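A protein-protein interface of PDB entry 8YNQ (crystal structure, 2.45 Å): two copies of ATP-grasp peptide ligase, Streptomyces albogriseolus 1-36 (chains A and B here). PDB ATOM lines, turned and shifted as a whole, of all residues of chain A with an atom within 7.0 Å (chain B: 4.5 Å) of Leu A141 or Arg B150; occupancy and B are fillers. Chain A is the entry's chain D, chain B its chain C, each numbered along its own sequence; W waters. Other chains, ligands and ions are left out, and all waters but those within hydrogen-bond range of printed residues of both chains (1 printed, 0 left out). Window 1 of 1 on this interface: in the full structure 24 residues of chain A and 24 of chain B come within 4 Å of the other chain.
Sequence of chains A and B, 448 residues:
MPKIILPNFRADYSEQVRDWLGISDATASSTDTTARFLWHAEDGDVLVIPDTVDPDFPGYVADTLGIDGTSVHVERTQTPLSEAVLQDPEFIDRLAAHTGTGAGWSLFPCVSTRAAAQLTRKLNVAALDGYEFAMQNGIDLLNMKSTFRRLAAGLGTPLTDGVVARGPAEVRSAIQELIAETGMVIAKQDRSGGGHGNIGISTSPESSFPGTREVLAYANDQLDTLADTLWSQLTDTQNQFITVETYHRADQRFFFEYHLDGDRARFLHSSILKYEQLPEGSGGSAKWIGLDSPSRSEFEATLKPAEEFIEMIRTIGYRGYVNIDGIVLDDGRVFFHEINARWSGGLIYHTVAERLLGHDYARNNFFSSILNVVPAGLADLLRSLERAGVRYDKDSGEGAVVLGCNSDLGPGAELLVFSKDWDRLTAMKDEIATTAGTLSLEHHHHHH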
ATOM      1  N   GLU A 132       0.317   8.680 -33.351  1.00  0.00           N
ATOM      2  CA  GLU A 132      -0.607   9.651 -33.932  1.00  0.00           C
ATOM      3  C   GLU A 132      -1.934   9.672 -33.193  1.00  0.00           C
ATOM      4  O   GLU A 132      -2.483  10.742 -32.921  1.00  0.00           O
ATOM      5  CB  GLU A 132      -0.832   9.361 -35.414  1.00  0.00           C
ATOM      6  CG  GLU A 132       0.420   8.966 -36.208  1.00  0.00           C
ATOM      7  CD  GLU A 132       1.490  10.068 -36.288  1.00  0.00           C
ATOM      8  OE1 GLU A 132       1.254  11.197 -35.804  1.00  0.00           O
ATOM      9  OE2 GLU A 132       2.582   9.801 -36.850  1.00  0.00           O
ATOM     10  N   PHE A 133      -2.487   8.506 -32.881  1.00  0.00           N
ATOM     11  CA  PHE A 133      -3.683   8.502 -32.050  1.00  0.00           C
ATOM     12  C   PHE A 133      -3.473   9.381 -30.824  1.00  0.00           C
ATOM     13  O   PHE A 133      -4.302  10.242 -30.507  1.00  0.00           O
ATOM     14  CB  PHE A 133      -4.022   7.072 -31.634  1.00  0.00           C
ATOM     15  CG  PHE A 133      -5.436   6.890 -31.120  1.00  0.00           C
ATOM     16  CD1 PHE A 133      -6.529   7.228 -31.904  1.00  0.00           C
ATOM     17  CD2 PHE A 133      -5.666   6.324 -29.870  1.00  0.00           C
ATOM     18  CE1 PHE A 133      -7.812   7.040 -31.443  1.00  0.00           C
ATOM     19  CE2 PHE A 133      -6.956   6.127 -29.408  1.00  0.00           C
ATOM     20  CZ  PHE A 133      -8.026   6.487 -30.194  1.00  0.00           C
ATOM     21  N   GLN A 136      -3.399  13.211 -31.232  1.00  0.00           N
ATOM     22  CA  GLN A 136      -4.721  13.791 -31.362  1.00  0.00           C
ATOM     23  C   GLN A 136      -5.544  13.604 -30.100  1.00  0.00           C
ATOM     24  O   GLN A 136      -6.770  13.730 -30.148  1.00  0.00           O
ATOM     25  CB  GLN A 136      -5.434  13.202 -32.575  1.00  0.00           C
ATOM     26  CG  GLN A 136      -4.737  13.538 -33.872  1.00  0.00           C
ATOM     27  CD  GLN A 136      -4.700  15.014 -34.096  1.00  0.00           C
ATOM     28  OE1 GLN A 136      -5.688  15.695 -33.877  1.00  0.00           O
ATOM     29  NE2 GLN A 136      -3.560  15.529 -34.526  1.00  0.00           N
ATOM     30  N   ASN A 137      -4.882  13.345 -28.968  1.00  0.00           N
ATOM     31  CA  ASN A 137      -5.539  13.126 -27.684  1.00  0.00           C
ATOM     32  C   ASN A 137      -6.559  12.006 -27.784  1.00  0.00           C
ATOM     33  O   ASN A 137      -7.593  12.011 -27.108  1.00  0.00           O
ATOM     34  CB  ASN A 137      -6.179  14.405 -27.161  1.00  0.00           C
ATOM     35  CG  ASN A 137      -5.151  15.496 -26.896  1.00  0.00           C
ATOM     36  OD1 ASN A 137      -4.296  15.359 -26.010  1.00  0.00           O
ATOM     37  ND2 ASN A 137      -5.223  16.586 -27.668  1.00  0.00           N
ATOM     38  N   GLY A 138      -6.240  11.031 -28.634  1.00  0.00           N
ATOM     39  CA  GLY A 138      -7.178   9.968 -28.915  1.00  0.00           C
ATOM     40  C   GLY A 138      -7.498   9.134 -27.697  1.00  0.00           C
ATOM     41  O   GLY A 138      -8.610   8.617 -27.563  1.00  0.00           O
ATOM     42  N   ILE A 139      -6.535   8.981 -26.787  1.00  0.00           N
ATOM     43  CA  ILE A 139      -6.782   8.070 -25.678  1.00  0.00           C
ATOM     44  C   ILE A 139      -7.735   8.683 -24.668  1.00  0.00           C
ATOM     45  O   ILE A 139      -8.174   7.987 -23.744  1.00  0.00           O
ATOM     46  CB  ILE A 139      -5.428   7.595 -25.108  1.00  0.00           C
ATOM     47  CG1 ILE A 139      -5.134   8.238 -23.772  1.00  0.00           C
ATOM     48  CG2 ILE A 139      -4.306   7.850 -26.121  1.00  0.00           C
ATOM     49  CD1 ILE A 139      -5.359   7.335 -22.650  1.00  0.00           C
ATOM     50  N   ASP A 140      -8.151   9.939 -24.880  1.00  0.00           N
ATOM     51  CA  ASP A 140      -9.130  10.595 -24.023  1.00  0.00           C
ATOM     52  C   ASP A 140     -10.580  10.452 -24.490  1.00  0.00           C
ATOM     53  O   ASP A 140     -11.486  10.665 -23.680  1.00  0.00           O
ATOM     54  CB  ASP A 140      -8.817  12.079 -23.888  1.00  0.00           C
ATOM     55  CG  ASP A 140      -9.728  12.761 -22.913  1.00  0.00           C
ATOM     56  OD1 ASP A 140      -9.916  12.193 -21.819  1.00  0.00           O
ATOM     57  OD2 ASP A 140     -10.285  13.831 -23.246  1.00  0.00           O
ATOM     58  N   LEU A 141     -10.854  10.095 -25.753  1.00  0.00           N
ATOM     59  CA  LEU A 141     -12.229   9.714 -26.090  1.00  0.00           C
ATOM     60  C   LEU A 141     -12.589   8.449 -25.364  1.00  0.00           C
ATOM     61  O   LEU A 141     -13.566   8.396 -24.613  1.00  0.00           O
ATOM     62  CB  LEU A 141     -12.450   9.464 -27.576  1.00  0.00           C
ATOM     63  CG  LEU A 141     -12.107  10.448 -28.653  1.00  0.00           C
ATOM     64  CD1 LEU A 141     -10.642  10.284 -28.844  1.00  0.00           C
ATOM     65  CD2 LEU A 141     -12.879  10.026 -29.899  1.00  0.00           C
ATOM     66  N   LEU A 142     -11.826   7.400 -25.626  1.00  0.00           N
ATOM     67  CA  LEU A 142     -11.752   6.283 -24.715  1.00  0.00           C
ATOM     68  C   LEU A 142     -11.406   6.865 -23.357  1.00  0.00           C
ATOM     69  O   LEU A 142     -10.878   7.971 -23.262  1.00  0.00           O
ATOM     70  CB  LEU A 142     -10.679   5.310 -25.203  1.00  0.00           C
ATOM     71  CG  LEU A 142     -10.463   5.339 -26.739  1.00  0.00           C
ATOM     72  CD1 LEU A 142      -9.431   4.322 -27.209  1.00  0.00           C
ATOM     73  CD2 LEU A 142     -11.742   5.162 -27.586  1.00  0.00           C
ATOM     74  N   ASN A 143     -11.715   6.142 -22.301  1.00  0.00           N
ATOM     75  CA  ASN A 143     -11.621   6.680 -20.947  1.00  0.00           C
ATOM     76  C   ASN A 143     -12.665   7.741 -20.702  1.00  0.00           C
ATOM     77  O   ASN A 143     -12.497   8.590 -19.818  1.00  0.00           O
ATOM     78  CB  ASN A 143     -10.247   7.273 -20.628  1.00  0.00           C
ATOM     79  CG  ASN A 143      -9.170   6.260 -20.715  1.00  0.00           C
ATOM     80  OD1 ASN A 143      -9.441   5.065 -20.795  1.00  0.00           O
ATOM     81  ND2 ASN A 143      -7.916   6.729 -20.781  1.00  0.00           N
ATOM     82  N   MET A 144     -13.707   7.741 -21.516  1.00  0.00           N
ATOM     83  CA  MET A 144     -14.960   8.382 -21.167  1.00  0.00           C
ATOM     84  C   MET A 144     -15.996   7.298 -20.997  1.00  0.00           C
ATOM     85  O   MET A 144     -16.053   6.359 -21.792  1.00  0.00           O
ATOM     86  CB  MET A 144     -15.446   9.349 -22.233  1.00  0.00           C
ATOM     87  CG  MET A 144     -14.477  10.404 -22.646  1.00  0.00           C
ATOM     88  SD  MET A 144     -15.327  11.352 -23.884  1.00  0.00           S
ATOM     89  CE  MET A 144     -14.069  12.493 -24.462  1.00  0.00           C
ATOM     90  N   LYS A 145     -16.827   7.428 -19.977  1.00  0.00           N
ATOM     91  CA  LYS A 145     -17.914   6.473 -19.884  1.00  0.00           C
ATOM     92  C   LYS A 145     -18.948   6.686 -20.997  1.00  0.00           C
ATOM     93  O   LYS A 145     -19.552   5.714 -21.475  1.00  0.00           O
ATOM     94  CB  LYS A 145     -18.512   6.530 -18.485  1.00  0.00           C
ATOM     95  CG  LYS A 145     -17.652   5.725 -17.486  1.00  0.00           C
ATOM     96  CD  LYS A 145     -17.814   6.191 -16.051  1.00  0.00           C
ATOM     97  CE  LYS A 145     -16.632   5.779 -15.165  1.00  0.00           C
ATOM     98  NZ  LYS A 145     -15.377   6.546 -15.428  1.00  0.00           N
ATOM     99  N   SER A 146     -19.123   7.926 -21.468  1.00  0.00           N
ATOM    100  CA  SER A 146     -20.030   8.163 -22.591  1.00  0.00           C
ATOM    101  C   SER A 146     -19.574   7.406 -23.834  1.00  0.00           C
ATOM    102  O   SER A 146     -20.351   6.648 -24.431  1.00  0.00           O
ATOM    103  CB  SER A 146     -20.123   9.649 -22.885  1.00  0.00           C
ATOM    104  OG  SER A 146     -18.821  10.189 -23.019  1.00  0.00           O
ATOM    105  N   THR A 147     -18.308   7.594 -24.235  1.00  0.00           N
ATOM    106  CA  THR A 147     -17.763   6.877 -25.384  1.00  0.00           C
ATOM    107  C   THR A 147     -17.981   5.372 -25.270  1.00  0.00           C
ATOM    108  O   THR A 147     -18.280   4.692 -26.266  1.00  0.00           O
ATOM    109  CB  THR A 147     -16.275   7.178 -25.530  1.00  0.00           C
ATOM    110  OG1 THR A 147     -16.096   8.583 -25.730  1.00  0.00           O
ATOM    111  CG2 THR A 147     -15.683   6.430 -26.720  1.00  0.00           C
ATOM    112  N   PHE A 148     -17.846   4.829 -24.062  1.00  0.00           N
ATOM    113  CA  PHE A 148     -17.948   3.388 -23.920  1.00  0.00           C
ATOM    114  C   PHE A 148     -19.321   2.910 -24.352  1.00  0.00           C
ATOM    115  O   PHE A 148     -19.441   2.130 -25.301  1.00  0.00           O
ATOM    116  CB  PHE A 148     -17.640   2.947 -22.493  1.00  0.00           C
ATOM    117  CG  PHE A 148     -17.734   1.474 -22.323  1.00  0.00           C
ATOM    118  CD1 PHE A 148     -16.749   0.648 -22.829  1.00  0.00           C
ATOM    119  CD2 PHE A 148     -18.858   0.904 -21.744  1.00  0.00           C
ATOM    120  CE1 PHE A 148     -16.868  -0.707 -22.718  1.00  0.00           C
ATOM    121  CE2 PHE A 148     -18.988  -0.458 -21.621  1.00  0.00           C
ATOM    122  CZ  PHE A 148     -18.002  -1.267 -22.111  1.00  0.00           C
ATOM    123  N   LEU A 151     -19.987   3.125 -27.944  1.00  0.00           N
ATOM    124  CA  LEU A 151     -19.285   2.120 -28.722  1.00  0.00           C
ATOM    125  C   LEU A 151     -19.898   0.747 -28.534  1.00  0.00           C
ATOM    126  O   LEU A 151     -19.881  -0.082 -29.458  1.00  0.00           O
ATOM    127  CB  LEU A 151     -17.827   2.085 -28.319  1.00  0.00           C
ATOM    128  CG  LEU A 151     -17.031   3.258 -28.832  1.00  0.00           C
ATOM    129  CD1 LEU A 151     -15.609   2.989 -28.424  1.00  0.00           C
ATOM    130  CD2 LEU A 151     -17.167   3.372 -30.339  1.00  0.00           C
ATOM    131  N   ASP A 190     -18.173  11.524 -16.349  1.00  0.00           N
ATOM    132  CA  ASP A 190     -17.760  10.947 -17.632  1.00  0.00           C
ATOM    133  C   ASP A 190     -16.283  10.578 -17.641  1.00  0.00           C
ATOM    134  O   ASP A 190     -15.914   9.494 -18.113  1.00  0.00           O
ATOM    135  CB  ASP A 190     -18.069  11.914 -18.784  1.00  0.00           C
ATOM    136  CG  ASP A 190     -18.341  11.190 -20.110  1.00  0.00           C
ATOM    137  OD1 ASP A 190     -18.541   9.949 -20.111  1.00  0.00           O
ATOM    138  OD2 ASP A 190     -18.336  11.863 -21.162  1.00  0.00           O
ATOM    139  N   ARG A 191     -15.423  11.466 -17.133  1.00  0.00           N
ATOM    140  CA  ARG A 191     -14.001  11.186 -16.935  1.00  0.00           C
ATOM    141  C   ARG A 191     -13.751  10.990 -15.448  1.00  0.00           C
ATOM    142  O   ARG A 191     -13.974  11.918 -14.661  1.00  0.00           O
ATOM    143  CB  ARG A 191     -13.134  12.329 -17.459  1.00  0.00           C
ATOM    144  CG  ARG A 191     -13.130  12.487 -18.970  1.00  0.00           C
ATOM    145  CD  ARG A 191     -12.625  13.852 -19.336  1.00  0.00           C
ATOM    146  NE  ARG A 191     -12.208  13.956 -20.725  1.00  0.00           N
ATOM    147  CZ  ARG A 191     -12.945  14.469 -21.701  1.00  0.00           C
ATOM    148  NH1 ARG A 191     -14.185  14.885 -21.494  1.00  0.00           N
ATOM    149  NH2 ARG A 191     -12.422  14.574 -22.918  1.00  0.00           N
ATOM    150  N   ILE A 316      -9.395   0.981 -33.996  1.00  0.00           N
ATOM    151  CA  ILE A 316      -9.432   2.437 -34.096  1.00  0.00           C
ATOM    152  C   ILE A 316      -8.102   3.085 -33.730  1.00  0.00           C
ATOM    153  O   ILE A 316      -7.913   4.278 -34.021  1.00  0.00           O
ATOM    154  CB  ILE A 316     -10.529   3.087 -33.236  1.00  0.00           C
ATOM    155  CG1 ILE A 316     -10.010   3.330 -31.840  1.00  0.00           C
ATOM    156  CG2 ILE A 316     -11.781   2.231 -33.185  1.00  0.00           C
ATOM    157  CD1 ILE A 316     -10.799   4.371 -31.116  1.00  0.00           C
ATOM    158  N   GLY A 317      -7.176   2.353 -33.096  1.00  0.00           N
ATOM    159  CA  GLY A 317      -5.800   2.837 -33.041  1.00  0.00           C
ATOM    160  C   GLY A 317      -5.008   2.712 -31.750  1.00  0.00           C
ATOM    161  O   GLY A 317      -3.772   2.778 -31.767  1.00  0.00           O
ATOM    162  N   ILE A 339     -13.986   0.637 -20.538  1.00  0.00           N
ATOM    163  CA  ILE A 339     -12.563   0.393 -20.715  1.00  0.00           C
ATOM    164  C   ILE A 339     -11.846   1.611 -20.164  1.00  0.00           C
ATOM    165  O   ILE A 339     -12.291   2.747 -20.355  1.00  0.00           O
ATOM    166  CB  ILE A 339     -12.131   0.163 -22.179  1.00  0.00           C
ATOM    167  CG1 ILE A 339     -12.719   1.228 -23.096  1.00  0.00           C
ATOM    168  CG2 ILE A 339     -12.499  -1.219 -22.649  1.00  0.00           C
ATOM    169  CD1 ILE A 339     -11.726   1.714 -24.122  1.00  0.00           C
ATOM    170  N   SER B 146     -13.271  16.651 -34.053  1.00  0.00           N
ATOM    171  CA  SER B 146     -12.222  16.058 -33.219  1.00  0.00           C
ATOM    172  C   SER B 146     -12.243  14.538 -33.292  1.00  0.00           C
ATOM    173  O   SER B 146     -11.192  13.890 -33.428  1.00  0.00           O
ATOM    174  CB  SER B 146     -12.381  16.509 -31.763  1.00  0.00           C
ATOM    175  OG  SER B 146     -13.716  16.329 -31.320  1.00  0.00           O
ATOM    176  N   THR B 147     -13.440  13.955 -33.205  1.00  0.00           N
ATOM    177  CA  THR B 147     -13.573  12.519 -33.357  1.00  0.00           C
ATOM    178  C   THR B 147     -12.911  12.062 -34.648  1.00  0.00           C
ATOM    179  O   THR B 147     -12.071  11.160 -34.646  1.00  0.00           O
ATOM    180  CB  THR B 147     -15.044  12.133 -33.328  1.00  0.00           C
ATOM    181  OG1 THR B 147     -15.627  12.527 -32.079  1.00  0.00           O
ATOM    182  CG2 THR B 147     -15.179  10.638 -33.493  1.00  0.00           C
ATOM    183  N   PHE B 148     -13.238  12.714 -35.762  1.00  0.00           N
ATOM    184  CA  PHE B 148     -12.672  12.256 -37.023  1.00  0.00           C
ATOM    185  C   PHE B 148     -11.156  12.304 -37.005  1.00  0.00           C
ATOM    186  O   PHE B 148     -10.496  11.369 -37.475  1.00  0.00           O
ATOM    187  CB  PHE B 148     -13.164  13.065 -38.210  1.00  0.00           C
ATOM    188  CG  PHE B 148     -12.545  12.596 -39.489  1.00  0.00           C
ATOM    189  CD1 PHE B 148     -12.982  11.422 -40.083  1.00  0.00           C
ATOM    190  CD2 PHE B 148     -11.472  13.264 -40.051  1.00  0.00           C
ATOM    191  CE1 PHE B 148     -12.409  10.943 -41.239  1.00  0.00           C
ATOM    192  CE2 PHE B 148     -10.888  12.792 -41.211  1.00  0.00           C
ATOM    193  CZ  PHE B 148     -11.364  11.625 -41.810  1.00  0.00           C
ATOM    194  N   ARG B 149     -10.578  13.392 -36.505  1.00  0.00           N
ATOM    195  CA  ARG B 149      -9.122  13.443 -36.459  1.00  0.00           C
ATOM    196  C   ARG B 149      -8.590  12.308 -35.621  1.00  0.00           C
ATOM    197  O   ARG B 149      -7.573  11.697 -35.953  1.00  0.00           O
ATOM    198  CB  ARG B 149      -8.650  14.785 -35.919  1.00  0.00           C
ATOM    199  CG  ARG B 149      -8.638  15.828 -37.004  1.00  0.00           C
ATOM    200  CD  ARG B 149      -7.640  16.920 -36.738  1.00  0.00           C
ATOM    201  NE  ARG B 149      -6.247  16.498 -36.819  1.00  0.00           N
ATOM    202  CZ  ARG B 149      -5.533  16.523 -37.936  1.00  0.00           C
ATOM    203  NH1 ARG B 149      -6.079  16.847 -39.103  1.00  0.00           N
ATOM    204  NH2 ARG B 149      -4.236  16.239 -37.881  1.00  0.00           N
ATOM    205  N   ARG B 150      -9.296  11.976 -34.556  1.00  0.00           N
ATOM    206  CA  ARG B 150      -8.806  10.927 -33.680  1.00  0.00           C
ATOM    207  C   ARG B 150      -8.838   9.574 -34.393  1.00  0.00           C
ATOM    208  O   ARG B 150      -7.792   8.952 -34.615  1.00  0.00           O
ATOM    209  CB  ARG B 150      -9.620  10.970 -32.382  1.00  0.00           C
ATOM    210  CG  ARG B 150      -9.208  12.199 -31.495  1.00  0.00           C
ATOM    211  CD  ARG B 150     -10.332  12.866 -30.670  1.00  0.00           C
ATOM    212  NE  ARG B 150      -9.842  13.305 -29.359  1.00  0.00           N
ATOM    213  CZ  ARG B 150     -10.588  13.720 -28.331  1.00  0.00           C
ATOM    214  NH1 ARG B 150     -11.911  13.713 -28.369  1.00  0.00           N
ATOM    215  NH2 ARG B 150      -9.984  14.162 -27.231  1.00  0.00           N
ATOM    216  N   LEU B 151     -10.023   9.144 -34.845  1.00  0.00           N
ATOM    217  CA  LEU B 151     -10.167   7.818 -35.449  1.00  0.00           C
ATOM    218  C   LEU B 151      -9.269   7.636 -36.663  1.00  0.00           C
ATOM    219  O   LEU B 151      -8.664   6.573 -36.843  1.00  0.00           O
ATOM    220  CB  LEU B 151     -11.603   7.601 -35.870  1.00  0.00           C
ATOM    221  CG  LEU B 151     -12.557   7.728 -34.717  1.00  0.00           C
ATOM    222  CD1 LEU B 151     -13.859   7.207 -35.223  1.00  0.00           C
ATOM    223  CD2 LEU B 151     -12.061   6.896 -33.580  1.00  0.00           C
ATOM    224  N   ALA B 152      -9.208   8.641 -37.533  1.00  0.00           N
ATOM    225  CA  ALA B 152      -8.399   8.495 -38.738  1.00  0.00           C
ATOM    226  C   ALA B 152      -6.932   8.377 -38.382  1.00  0.00           C
ATOM    227  O   ALA B 152      -6.214   7.529 -38.925  1.00  0.00           O
ATOM    228  CB  ALA B 152      -8.611   9.684 -39.669  1.00  0.00           C
ATOM    229  N   ALA B 153      -6.473   9.233 -37.472  1.00  0.00           N
ATOM    230  CA  ALA B 153      -5.097   9.178 -37.031  1.00  0.00           C
ATOM    231  C   ALA B 153      -4.777   7.841 -36.376  1.00  0.00           C
ATOM    232  O   ALA B 153      -3.615   7.427 -36.377  1.00  0.00           O
ATOM    233  CB  ALA B 153      -4.829  10.336 -36.073  1.00  0.00           C
ATOM    234  N   GLY B 154      -5.778   7.156 -35.824  1.00  0.00           N
ATOM    235  CA  GLY B 154      -5.539   5.861 -35.229  1.00  0.00           C
ATOM    236  C   GLY B 154      -5.608   4.783 -36.284  1.00  0.00           C
ATOM    237  O   GLY B 154      -4.860   3.796 -36.253  1.00  0.00           O
ATOM    238  N   VAL B 164      -6.118  18.429 -32.072  1.00  0.00           N
ATOM    239  CA  VAL B 164      -7.325  18.654 -31.283  1.00  0.00           C
ATOM    240  C   VAL B 164      -6.946  19.609 -30.150  1.00  0.00           C
ATOM    241  O   VAL B 164      -6.406  19.199 -29.121  1.00  0.00           O
ATOM    242  CB  VAL B 164      -7.923  17.352 -30.753  1.00  0.00           C
ATOM    243  CG1 VAL B 164      -9.231  17.647 -30.072  1.00  0.00           C
ATOM    244  CG2 VAL B 164      -8.134  16.352 -31.881  1.00  0.00           C
ATOM    245  N   PHE B 241     -13.373  21.613 -27.685  1.00  0.00           N
ATOM    246  CA  PHE B 241     -12.343  21.283 -28.653  1.00  0.00           C
ATOM    247  C   PHE B 241     -12.459  22.214 -29.845  1.00  0.00           C
ATOM    248  O   PHE B 241     -13.573  22.528 -30.291  1.00  0.00           O
ATOM    249  CB  PHE B 241     -12.456  19.826 -29.143  1.00  0.00           C
ATOM    250  CG  PHE B 241     -12.266  18.799 -28.065  1.00  0.00           C
ATOM    251  CD1 PHE B 241     -11.192  18.868 -27.200  1.00  0.00           C
ATOM    252  CD2 PHE B 241     -13.166  17.749 -27.920  1.00  0.00           C
ATOM    253  CE1 PHE B 241     -11.021  17.898 -26.186  1.00  0.00           C
ATOM    254  CE2 PHE B 241     -13.006  16.785 -26.906  1.00  0.00           C
ATOM    255  CZ  PHE B 241     -11.936  16.857 -26.043  1.00  0.00           C
HETATM  256  O   HOH W   1      -2.580   3.664 -34.291  1.00  0.00           O
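OE1 of Gln A136 sits at hydrogen-bond distance from NE of Arg B149, at 3.1 Å.
The backbone carbonyl oxygen (O) of Gln A136 sits close to the guanidinium group (NE) of Arg B150 (3.2 Å).
O of Asn A137 lies within hydrogen-bond range of NH2 of Arg B150 (3.2 Å).
OE1 of Gln A136 sits close to N of Val B164 (3.3 Å).
ND2 of Asn A137 is in hydrogen-bond range of O of Val B164 (3.2 Å).
The backbone carbonyl oxygen (O) of Phe A133 lies within hydrogen-bond range of the backbone NH (N) of Gly A138 (2.8 Å).
The side-chain carboxylate (OD1) of Asp A140 is in salt-bridge range of the guanidinium group (NE) of Arg A191 (3.1 Å).
O of Leu A141 is in hydrogen-bond range of OG1 of Thr A147 (2.8 Å).
Among the printed residues, pairs that only touch across the chains: Ile A316 with Gly B154, Leu A141 with Arg B150, Phe A133 with Arg B150, Gly A317 with Gly B154, Glu A132 with Ala B153, Ile A316 with Leu B151, Phe A133 with Gly B154, Phe A133 with Ala B153, Gln A136 with Ala B153, Arg A191 with Phe B241 and Gly A138 with Arg B150.
Of the printed residues of chain B, Leu A141 touches Arg B150 (3.2 Å).
Of the printed residues of chain A, Arg B150 touches Phe A133 (3.5 Å), Gln A136 (3.2 Å), Asn A137 (3.2 Å), Gly A138 (3.97 Å) and Leu A141 (3.2 Å).
Of the printed residues of chain B, Phe A133 touches Arg B150, Ala B153 and Gly B154.
Of the printed residues of chain B, Gly A138 touches Arg B150 (3.97 Å).
Printed residues of chain B within 4 Å of Gly A317: Gly B154.
Thr B147 touches none of the printed residues of chain A.
Of the 21 printed residues of chain A, 9 touch a printed residue of chain B.
Hydrophobic or aromatic side chains of chain A within 4 Å of the printed part of chain B: Phe A133, Leu A141 and Ile A316.
Printed residues of chain B that touch a printed residue of chain A: Arg B149, Arg B150, Leu B151, Ala B153, Gly B154, Val B164 and Phe B241.
Hydrophobic or aromatic side chains of chain B within 4 Å of the printed part of chain A: Leu B151, Ala B153, Val B164 and Phe B241.
Among the printed residues, 16 pairs touch across the chains.
Among the printed residues, no Asp or Glu carboxylate lies within 4 Å of a Lys or Arg side-chain nitrogen of the other chain.
4 positions are printed for both chains.
Water W1 lies within hydrogen-bond range of O of Gly A317 (2.9 Å) and O of Gly B154 (3.0 Å).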
